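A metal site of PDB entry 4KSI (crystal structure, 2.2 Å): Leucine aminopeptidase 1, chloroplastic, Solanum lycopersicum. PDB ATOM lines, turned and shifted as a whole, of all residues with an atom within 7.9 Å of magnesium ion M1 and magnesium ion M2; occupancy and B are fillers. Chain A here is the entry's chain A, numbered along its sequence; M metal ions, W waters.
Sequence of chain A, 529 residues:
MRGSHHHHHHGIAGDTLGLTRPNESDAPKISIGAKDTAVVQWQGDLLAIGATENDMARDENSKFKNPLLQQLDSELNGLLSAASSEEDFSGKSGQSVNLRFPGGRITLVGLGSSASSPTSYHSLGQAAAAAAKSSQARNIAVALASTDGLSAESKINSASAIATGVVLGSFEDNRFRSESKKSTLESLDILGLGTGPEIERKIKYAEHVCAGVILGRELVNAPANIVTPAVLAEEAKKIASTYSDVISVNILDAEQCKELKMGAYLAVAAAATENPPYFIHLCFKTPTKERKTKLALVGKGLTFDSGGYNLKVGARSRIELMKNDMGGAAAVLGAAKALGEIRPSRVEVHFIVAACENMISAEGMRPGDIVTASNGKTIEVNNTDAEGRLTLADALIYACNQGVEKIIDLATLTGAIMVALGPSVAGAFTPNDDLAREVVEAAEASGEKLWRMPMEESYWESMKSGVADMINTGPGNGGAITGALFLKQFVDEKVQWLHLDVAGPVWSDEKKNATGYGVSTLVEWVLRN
Merely in contact with magnesium ion M2: Lys 312 (3.9 Å).
Four residues have an atom within 4 Å of magnesium ion M2: Asp 305, Lys 312, Asp 385 and Glu 387.
Water W2 bridges the side-chain carboxylate of Asp 325 (2.9 Å) and the side-chain sulfur of Met 322 (3.7 Å).
The backbone NH of Asp 385 lies within hydrogen-bond range of the side-chain amide oxygen of Asn 383 (2.8 Å).
The backbone NH (N) of Asp 385 lies within hydrogen-bond range of the backbone carbonyl oxygen (O) of Gly 307 (3.3 Å).
The side-chain amide nitrogen of Asn 358 is in hydrogen-bond range of the side-chain carboxylate of Asp 305, 2.8 Å away.
The backbone carbonyl oxygen of Thr 412 lies close to the side-chain amino group of Lys 300.
N of Leu 302 lies within hydrogen-bond range of O of Asp 325, 3.3 Å away.
The side-chain carboxylate of Asp 325 is in hydrogen-bond range of the side-chain hydroxyl of Thr 412 (2.7 Å).
OD2 of Asp 305 sits close to NZ of Lys 312 (3.7 Å).
The backbone NH (N) of Lys 312 lies within hydrogen-bond range of the backbone carbonyl oxygen (O) of Ser 306 (3.0 Å).
Magnesium ion M2 is bound by water W1 (1.8 Å), OE1 of Glu 387 (2.0 Å), OD2 of Asp 305 (2.0 Å), OD1 of Asp 385 (2.1 Å) and O of Asp 385 (2.3 Å).
Magnesium ion M1 is bound by the side-chain carboxylate (OD2) of Asp 325 (2.0 Å), the side-chain carboxylate (OE2) of Glu 387 (2.1 Å), the side-chain amino group (NZ) of Lys 300 (2.3 Å) and water W1 (2.5 Å).
Slightly farther from magnesium ion M1 lies OD2 of Asp 305 (2.7 Å).
Slightly farther from magnesium ion M1 lies water W2 (2.7 Å).
Of the 27 residues printed, 4 come within 4 Å of magnesium ion M1.
The nearest printed residue that does not touch magnesium ion M1 is Leu 302 (4.4 Å).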
ATOM      1  N   VAL A 268      28.940 -22.445  -0.503  1.00  0.00           N
ATOM      2  CA  VAL A 268      28.469 -23.125   0.723  1.00  0.00           C
ATOM      3  C   VAL A 268      26.936 -23.246   0.656  1.00  0.00           C
ATOM      4  O   VAL A 268      26.354 -24.325   0.945  1.00  0.00           O
ATOM      5  CB  VAL A 268      28.850 -22.346   2.011  1.00  0.00           C
ATOM      6  CG1 VAL A 268      28.188 -23.003   3.222  1.00  0.00           C
ATOM      7  CG2 VAL A 268      30.387 -22.248   2.153  1.00  0.00           C
ATOM      8  N   LYS A 300      29.428 -15.436  12.070  1.00  0.00           N
ATOM      9  CA  LYS A 300      29.211 -16.587  11.253  1.00  0.00           C
ATOM     10  C   LYS A 300      27.746 -16.975  11.415  1.00  0.00           C
ATOM     11  O   LYS A 300      27.260 -17.142  12.544  1.00  0.00           O
ATOM     12  CB  LYS A 300      30.093 -17.740  11.741  1.00  0.00           C
ATOM     13  CG  LYS A 300      29.810 -19.044  10.990  1.00  0.00           C
ATOM     14  CD  LYS A 300      30.624 -20.213  11.568  1.00  0.00           C
ATOM     15  CE  LYS A 300      30.118 -21.523  11.006  1.00  0.00           C
ATOM     16  NZ  LYS A 300      30.897 -22.655  11.583  1.00  0.00           N
ATOM     17  N   GLY A 301      27.043 -17.111  10.297  1.00  0.00           N
ATOM     18  CA  GLY A 301      25.614 -17.315  10.369  1.00  0.00           C
ATOM     19  C   GLY A 301      25.150 -18.574   9.641  1.00  0.00           C
ATOM     20  O   GLY A 301      24.263 -18.535   8.779  1.00  0.00           O
ATOM     21  N   LEU A 302      25.714 -19.702  10.053  1.00  0.00           N
ATOM     22  CA  LEU A 302      25.259 -21.001   9.544  1.00  0.00           C
ATOM     23  C   LEU A 302      24.059 -21.409  10.408  1.00  0.00           C
ATOM     24  O   LEU A 302      24.227 -21.947  11.542  1.00  0.00           O
ATOM     25  CB  LEU A 302      26.414 -22.049   9.608  1.00  0.00           C
ATOM     26  CG  LEU A 302      27.304 -22.139   8.341  1.00  0.00           C
ATOM     27  CD1 LEU A 302      26.553 -22.820   7.180  1.00  0.00           C
ATOM     28  CD2 LEU A 302      27.686 -20.730   7.858  1.00  0.00           C
ATOM     29  N   PHE A 304      22.177 -23.862  10.040  1.00  0.00           N
ATOM     30  CA  PHE A 304      22.438 -25.278  10.313  1.00  0.00           C
ATOM     31  C   PHE A 304      23.675 -25.711   9.548  1.00  0.00           C
ATOM     32  O   PHE A 304      23.924 -25.256   8.428  1.00  0.00           O
ATOM     33  CB  PHE A 304      21.282 -26.228   9.944  1.00  0.00           C
ATOM     34  CG  PHE A 304      21.516 -27.624  10.455  1.00  0.00           C
ATOM     35  CD1 PHE A 304      21.433 -27.903  11.833  1.00  0.00           C
ATOM     36  CD2 PHE A 304      21.970 -28.633   9.597  1.00  0.00           C
ATOM     37  CE1 PHE A 304      21.762 -29.180  12.337  1.00  0.00           C
ATOM     38  CE2 PHE A 304      22.246 -29.899  10.067  1.00  0.00           C
ATOM     39  CZ  PHE A 304      22.148 -30.169  11.450  1.00  0.00           C
ATOM     40  N   ASP A 305      24.431 -26.661  10.110  1.00  0.00           N
ATOM     41  CA  ASP A 305      25.614 -27.166   9.425  1.00  0.00           C
ATOM     42  C   ASP A 305      25.612 -28.678   9.507  1.00  0.00           C
ATOM     43  O   ASP A 305      25.909 -29.264  10.571  1.00  0.00           O
ATOM     44  CB  ASP A 305      26.893 -26.624  10.071  1.00  0.00           C
ATOM     45  CG  ASP A 305      28.168 -27.143   9.396  1.00  0.00           C
ATOM     46  OD1 ASP A 305      28.117 -27.659   8.247  1.00  0.00           O
ATOM     47  OD2 ASP A 305      29.261 -27.045  10.039  1.00  0.00           O
ATOM     48  N   SER A 306      25.262 -29.338   8.390  1.00  0.00           N
ATOM     49  CA  SER A 306      25.339 -30.794   8.352  1.00  0.00           C
ATOM     50  C   SER A 306      26.804 -31.232   8.128  1.00  0.00           C
ATOM     51  O   SER A 306      27.098 -32.368   8.290  1.00  0.00           O
ATOM     52  CB  SER A 306      24.467 -31.374   7.215  1.00  0.00           C
ATOM     53  OG  SER A 306      24.990 -30.955   5.931  1.00  0.00           O
ATOM     54  N   GLY A 307      27.692 -30.326   7.685  1.00  0.00           N
ATOM     55  CA  GLY A 307      29.007 -30.761   7.162  1.00  0.00           C
ATOM     56  C   GLY A 307      29.024 -30.785   5.639  1.00  0.00           C
ATOM     57  O   GLY A 307      30.102 -30.742   5.025  1.00  0.00           O
ATOM     58  N   GLY A 308      27.840 -30.827   4.984  1.00  0.00           N
ATOM     59  CA  GLY A 308      27.779 -30.936   3.508  1.00  0.00           C
ATOM     60  C   GLY A 308      28.250 -32.343   3.154  1.00  0.00           C
ATOM     61  O   GLY A 308      28.107 -33.284   3.975  1.00  0.00           O
ATOM     62  N   ASN A 310      31.083 -33.634   3.264  1.00  0.00           N
ATOM     63  CA  ASN A 310      31.873 -34.082   4.399  1.00  0.00           C
ATOM     64  C   ASN A 310      30.937 -34.114   5.620  1.00  0.00           C
ATOM     65  O   ASN A 310      31.143 -33.403   6.631  1.00  0.00           O
ATOM     66  CB  ASN A 310      33.056 -33.122   4.604  1.00  0.00           C
ATOM     67  CG  ASN A 310      34.228 -33.408   3.628  1.00  0.00           C
ATOM     68  OD1 ASN A 310      35.008 -34.410   3.802  1.00  0.00           O
ATOM     69  ND2 ASN A 310      34.380 -32.557   2.665  1.00  0.00           N
ATOM     70  N   LYS A 312      28.971 -34.559   8.969  1.00  0.00           N
ATOM     71  CA  LYS A 312      29.304 -34.807  10.383  1.00  0.00           C
ATOM     72  C   LYS A 312      28.840 -36.197  10.834  1.00  0.00           C
ATOM     73  O   LYS A 312      27.642 -36.489  10.862  1.00  0.00           O
ATOM     74  CB  LYS A 312      28.640 -33.721  11.222  1.00  0.00           C
ATOM     75  CG  LYS A 312      29.277 -32.346  11.053  1.00  0.00           C
ATOM     76  CD  LYS A 312      28.507 -31.278  11.826  1.00  0.00           C
ATOM     77  CE  LYS A 312      29.069 -29.862  11.570  1.00  0.00           C
ATOM     78  NZ  LYS A 312      30.529 -29.862  11.991  1.00  0.00           N
ATOM     79  N   MET A 322      23.820 -28.445  15.750  1.00  0.00           N
ATOM     80  CA  MET A 322      24.381 -27.485  14.777  1.00  0.00           C
ATOM     81  C   MET A 322      23.465 -26.320  14.396  1.00  0.00           C
ATOM     82  O   MET A 322      23.860 -25.449  13.604  1.00  0.00           O
ATOM     83  CB  MET A 322      24.985 -28.174  13.539  1.00  0.00           C
ATOM     84  CG  MET A 322      26.263 -29.003  13.806  1.00  0.00           C
ATOM     85  SD  MET A 322      27.595 -27.961  14.503  1.00  0.00           S
ATOM     86  CE  MET A 322      27.498 -28.273  16.291  1.00  0.00           C
ATOM     87  N   ASN A 324      23.351 -24.278  16.455  1.00  0.00           N
ATOM     88  CA  ASN A 324      24.083 -23.233  17.167  1.00  0.00           C
ATOM     89  C   ASN A 324      25.298 -22.737  16.371  1.00  0.00           C
ATOM     90  O   ASN A 324      26.093 -21.920  16.878  1.00  0.00           O
ATOM     91  CB  ASN A 324      24.508 -23.689  18.556  1.00  0.00           C
ATOM     92  CG  ASN A 324      25.569 -24.730  18.509  1.00  0.00           C
ATOM     93  OD1 ASN A 324      26.153 -24.972  17.455  1.00  0.00           O
ATOM     94  ND2 ASN A 324      25.829 -25.355  19.647  1.00  0.00           N
ATOM     95  N   ASP A 325      25.416 -23.213  15.129  1.00  0.00           N
ATOM     96  CA  ASP A 325      26.483 -22.716  14.256  1.00  0.00           C
ATOM     97  C   ASP A 325      26.222 -21.303  13.737  1.00  0.00           C
ATOM     98  O   ASP A 325      27.004 -20.782  12.932  1.00  0.00           O
ATOM     99  CB  ASP A 325      26.645 -23.680  13.099  1.00  0.00           C
ATOM    100  CG  ASP A 325      28.112 -23.985  12.811  1.00  0.00           C
ATOM    101  OD1 ASP A 325      29.001 -23.951  13.726  1.00  0.00           O
ATOM    102  OD2 ASP A 325      28.377 -24.282  11.619  1.00  0.00           O
ATOM    103  N   MET A 326      25.089 -20.731  14.130  1.00  0.00           N
ATOM    104  CA  MET A 326      24.865 -19.286  13.904  1.00  0.00           C
ATOM    105  C   MET A 326      25.083 -18.510  15.243  1.00  0.00           C
ATOM    106  O   MET A 326      24.685 -17.358  15.362  1.00  0.00           O
ATOM    107  CB  MET A 326      23.488 -18.967  13.253  1.00  0.00           C
ATOM    108  CG  MET A 326      22.303 -19.805  13.742  1.00  0.00           C
ATOM    109  SD  MET A 326      22.111 -19.529  15.524  1.00  0.00           S
ATOM    110  CE  MET A 326      21.481 -17.815  15.577  1.00  0.00           C
ATOM    111  N   ASN A 358      24.162 -25.330   5.572  1.00  0.00           N
ATOM    112  CA  ASN A 358      25.139 -26.136   4.836  1.00  0.00           C
ATOM    113  C   ASN A 358      24.514 -27.548   4.723  1.00  0.00           C
ATOM    114  O   ASN A 358      24.503 -28.304   5.711  1.00  0.00           O
ATOM    115  CB  ASN A 358      26.476 -26.205   5.621  1.00  0.00           C
ATOM    116  CG  ASN A 358      27.632 -26.910   4.828  1.00  0.00           C
ATOM    117  OD1 ASN A 358      27.615 -26.942   3.591  1.00  0.00           O
ATOM    118  ND2 ASN A 358      28.650 -27.424   5.536  1.00  0.00           N
ATOM    119  N   ASN A 383      37.629 -29.811   2.477  1.00  0.00           N
ATOM    120  CA  ASN A 383      36.645 -30.376   3.424  1.00  0.00           C
ATOM    121  C   ASN A 383      35.438 -29.457   3.476  1.00  0.00           C
ATOM    122  O   ASN A 383      35.597 -28.288   3.815  1.00  0.00           O
ATOM    123  CB  ASN A 383      37.256 -30.558   4.847  1.00  0.00           C
ATOM    124  CG  ASN A 383      36.337 -31.369   5.797  1.00  0.00           C
ATOM    125  OD1 ASN A 383      35.107 -31.153   5.872  1.00  0.00           O
ATOM    126  ND2 ASN A 383      36.948 -32.308   6.564  1.00  0.00           N
ATOM    127  N   THR A 384      34.271 -29.926   3.096  1.00  0.00           N
ATOM    128  CA  THR A 384      33.120 -29.022   3.031  1.00  0.00           C
ATOM    129  C   THR A 384      32.559 -28.692   4.388  1.00  0.00           C
ATOM    130  O   THR A 384      31.636 -27.882   4.489  1.00  0.00           O
ATOM    131  CB  THR A 384      31.951 -29.595   2.168  1.00  0.00           C
ATOM    132  OG1 THR A 384      31.440 -30.780   2.807  1.00  0.00           O
ATOM    133  CG2 THR A 384      32.450 -29.942   0.732  1.00  0.00           C
ATOM    134  N   ASP A 385      33.072 -29.350   5.419  1.00  0.00           N
ATOM    135  CA  ASP A 385      32.646 -29.058   6.771  1.00  0.00           C
ATOM    136  C   ASP A 385      33.491 -27.916   7.395  1.00  0.00           C
ATOM    137  O   ASP A 385      33.302 -27.527   8.562  1.00  0.00           O
ATOM    138  CB  ASP A 385      32.711 -30.313   7.643  1.00  0.00           C
ATOM    139  CG  ASP A 385      31.991 -30.114   8.998  1.00  0.00           C
ATOM    140  OD1 ASP A 385      31.202 -29.110   9.208  1.00  0.00           O
ATOM    141  OD2 ASP A 385      32.186 -30.947   9.864  1.00  0.00           O
ATOM    142  N   ALA A 386      34.439 -27.367   6.635  1.00  0.00           N
ATOM    143  CA  ALA A 386      35.087 -26.152   7.061  1.00  0.00           C
ATOM    144  C   ALA A 386      34.506 -25.008   6.193  1.00  0.00           C
ATOM    145  O   ALA A 386      35.236 -24.276   5.505  1.00  0.00           O
ATOM    146  CB  ALA A 386      36.630 -26.281   6.943  1.00  0.00           C
ATOM    147  N   GLU A 387      33.176 -24.848   6.263  1.00  0.00           N
ATOM    148  CA  GLU A 387      32.419 -23.997   5.337  1.00  0.00           C
ATOM    149  C   GLU A 387      32.218 -22.614   5.931  1.00  0.00           C
ATOM    150  O   GLU A 387      32.021 -21.639   5.224  1.00  0.00           O
ATOM    151  CB  GLU A 387      31.023 -24.637   5.059  1.00  0.00           C
ATOM    152  CG  GLU A 387      29.974 -24.431   6.189  1.00  0.00           C
ATOM    153  CD  GLU A 387      30.365 -25.051   7.535  1.00  0.00           C
ATOM    154  OE1 GLU A 387      30.904 -26.202   7.615  1.00  0.00           O
ATOM    155  OE2 GLU A 387      30.154 -24.372   8.574  1.00  0.00           O
ATOM    156  N   GLY A 388      32.304 -22.520   7.258  1.00  0.00           N
ATOM    157  CA  GLY A 388      32.072 -21.228   7.911  1.00  0.00           C
ATOM    158  C   GLY A 388      33.115 -20.220   7.501  1.00  0.00           C
ATOM    159  O   GLY A 388      32.792 -19.026   7.235  1.00  0.00           O
ATOM    160  N   ARG A 389      34.367 -20.667   7.391  1.00  0.00           N
ATOM    161  CA  ARG A 389      35.409 -19.732   6.974  1.00  0.00           C
ATOM    162  C   ARG A 389      35.215 -19.235   5.512  1.00  0.00           C
ATOM    163  O   ARG A 389      35.694 -18.155   5.181  1.00  0.00           O
ATOM    164  CB  ARG A 389      36.799 -20.359   7.168  1.00  0.00           C
ATOM    165  CG  ARG A 389      37.028 -21.582   6.247  1.00  0.00           C
ATOM    166  CD  ARG A 389      38.229 -22.419   6.796  1.00  0.00           C
ATOM    167  NE  ARG A 389      37.914 -23.005   8.095  1.00  0.00           N
ATOM    168  CZ  ARG A 389      38.800 -23.643   8.875  1.00  0.00           C
ATOM    169  NH1 ARG A 389      40.084 -23.822   8.465  1.00  0.00           N
ATOM    170  NH2 ARG A 389      38.399 -24.152  10.013  1.00  0.00           N
ATOM    171  N   THR A 391      32.131 -18.674   4.099  1.00  0.00           N
ATOM    172  CA  THR A 391      31.130 -17.607   4.184  1.00  0.00           C
ATOM    173  C   THR A 391      31.755 -16.353   4.808  1.00  0.00           C
ATOM    174  O   THR A 391      31.472 -15.245   4.370  1.00  0.00           O
ATOM    175  CB  THR A 391      29.889 -18.029   4.966  1.00  0.00           C
ATOM    176  OG1 THR A 391      30.223 -18.114   6.341  1.00  0.00           O
ATOM    177  CG2 THR A 391      29.420 -19.393   4.502  1.00  0.00           C
ATOM    178  N   THR A 412      31.588 -19.762  15.507  1.00  0.00           N
ATOM    179  CA  THR A 412      31.725 -21.147  15.996  1.00  0.00           C
ATOM    180  C   THR A 412      32.608 -21.953  15.033  1.00  0.00           C
ATOM    181  O   THR A 412      32.090 -22.714  14.238  1.00  0.00           O
ATOM    182  CB  THR A 412      30.356 -21.829  16.080  1.00  0.00           C
ATOM    183  OG1 THR A 412      29.628 -21.548  14.885  1.00  0.00           O
ATOM    184  CG2 THR A 412      29.534 -21.204  17.280  1.00  0.00           C
ATOM    185  N   LEU A 413      33.903 -21.729  15.016  1.00  0.00           N
ATOM    186  CA  LEU A 413      34.652 -22.160  13.860  1.00  0.00           C
ATOM    187  C   LEU A 413      35.180 -23.577  13.991  1.00  0.00           C
ATOM    188  O   LEU A 413      35.086 -24.349  13.047  1.00  0.00           O
ATOM    189  CB  LEU A 413      35.825 -21.210  13.549  1.00  0.00           C
ATOM    190  CG  LEU A 413      36.171 -21.122  12.033  1.00  0.00           C
ATOM    191  CD1 LEU A 413      35.174 -20.223  11.275  1.00  0.00           C
ATOM    192  CD2 LEU A 413      37.597 -20.601  11.802  1.00  0.00           C
ATOM    193  N   THR A 414      35.757 -23.942  15.131  1.00  0.00           N
ATOM    194  CA  THR A 414      36.537 -25.200  15.143  1.00  0.00           C
ATOM    195  C   THR A 414      36.251 -26.004  16.409  1.00  0.00           C
ATOM    196  O   THR A 414      36.047 -25.395  17.501  1.00  0.00           O
ATOM    197  CB  THR A 414      38.081 -24.987  15.009  1.00  0.00           C
ATOM    198  OG1 THR A 414      38.574 -24.313  16.185  1.00  0.00           O
ATOM    199  CG2 THR A 414      38.429 -24.149  13.771  1.00  0.00           C
HETATM  200 MG    MG M   1      30.080 -24.595  10.664  1.00  0.00          MG
HETATM  201 MG    MG M   2      31.209 -27.049   9.409  1.00  0.00          MG
HETATM  202  O   HOH W   1      31.967 -26.207  10.830  1.00  0.00           O
HETATM  203  O   HOH W   2      30.404 -26.281  12.708  1.00  0.00           O
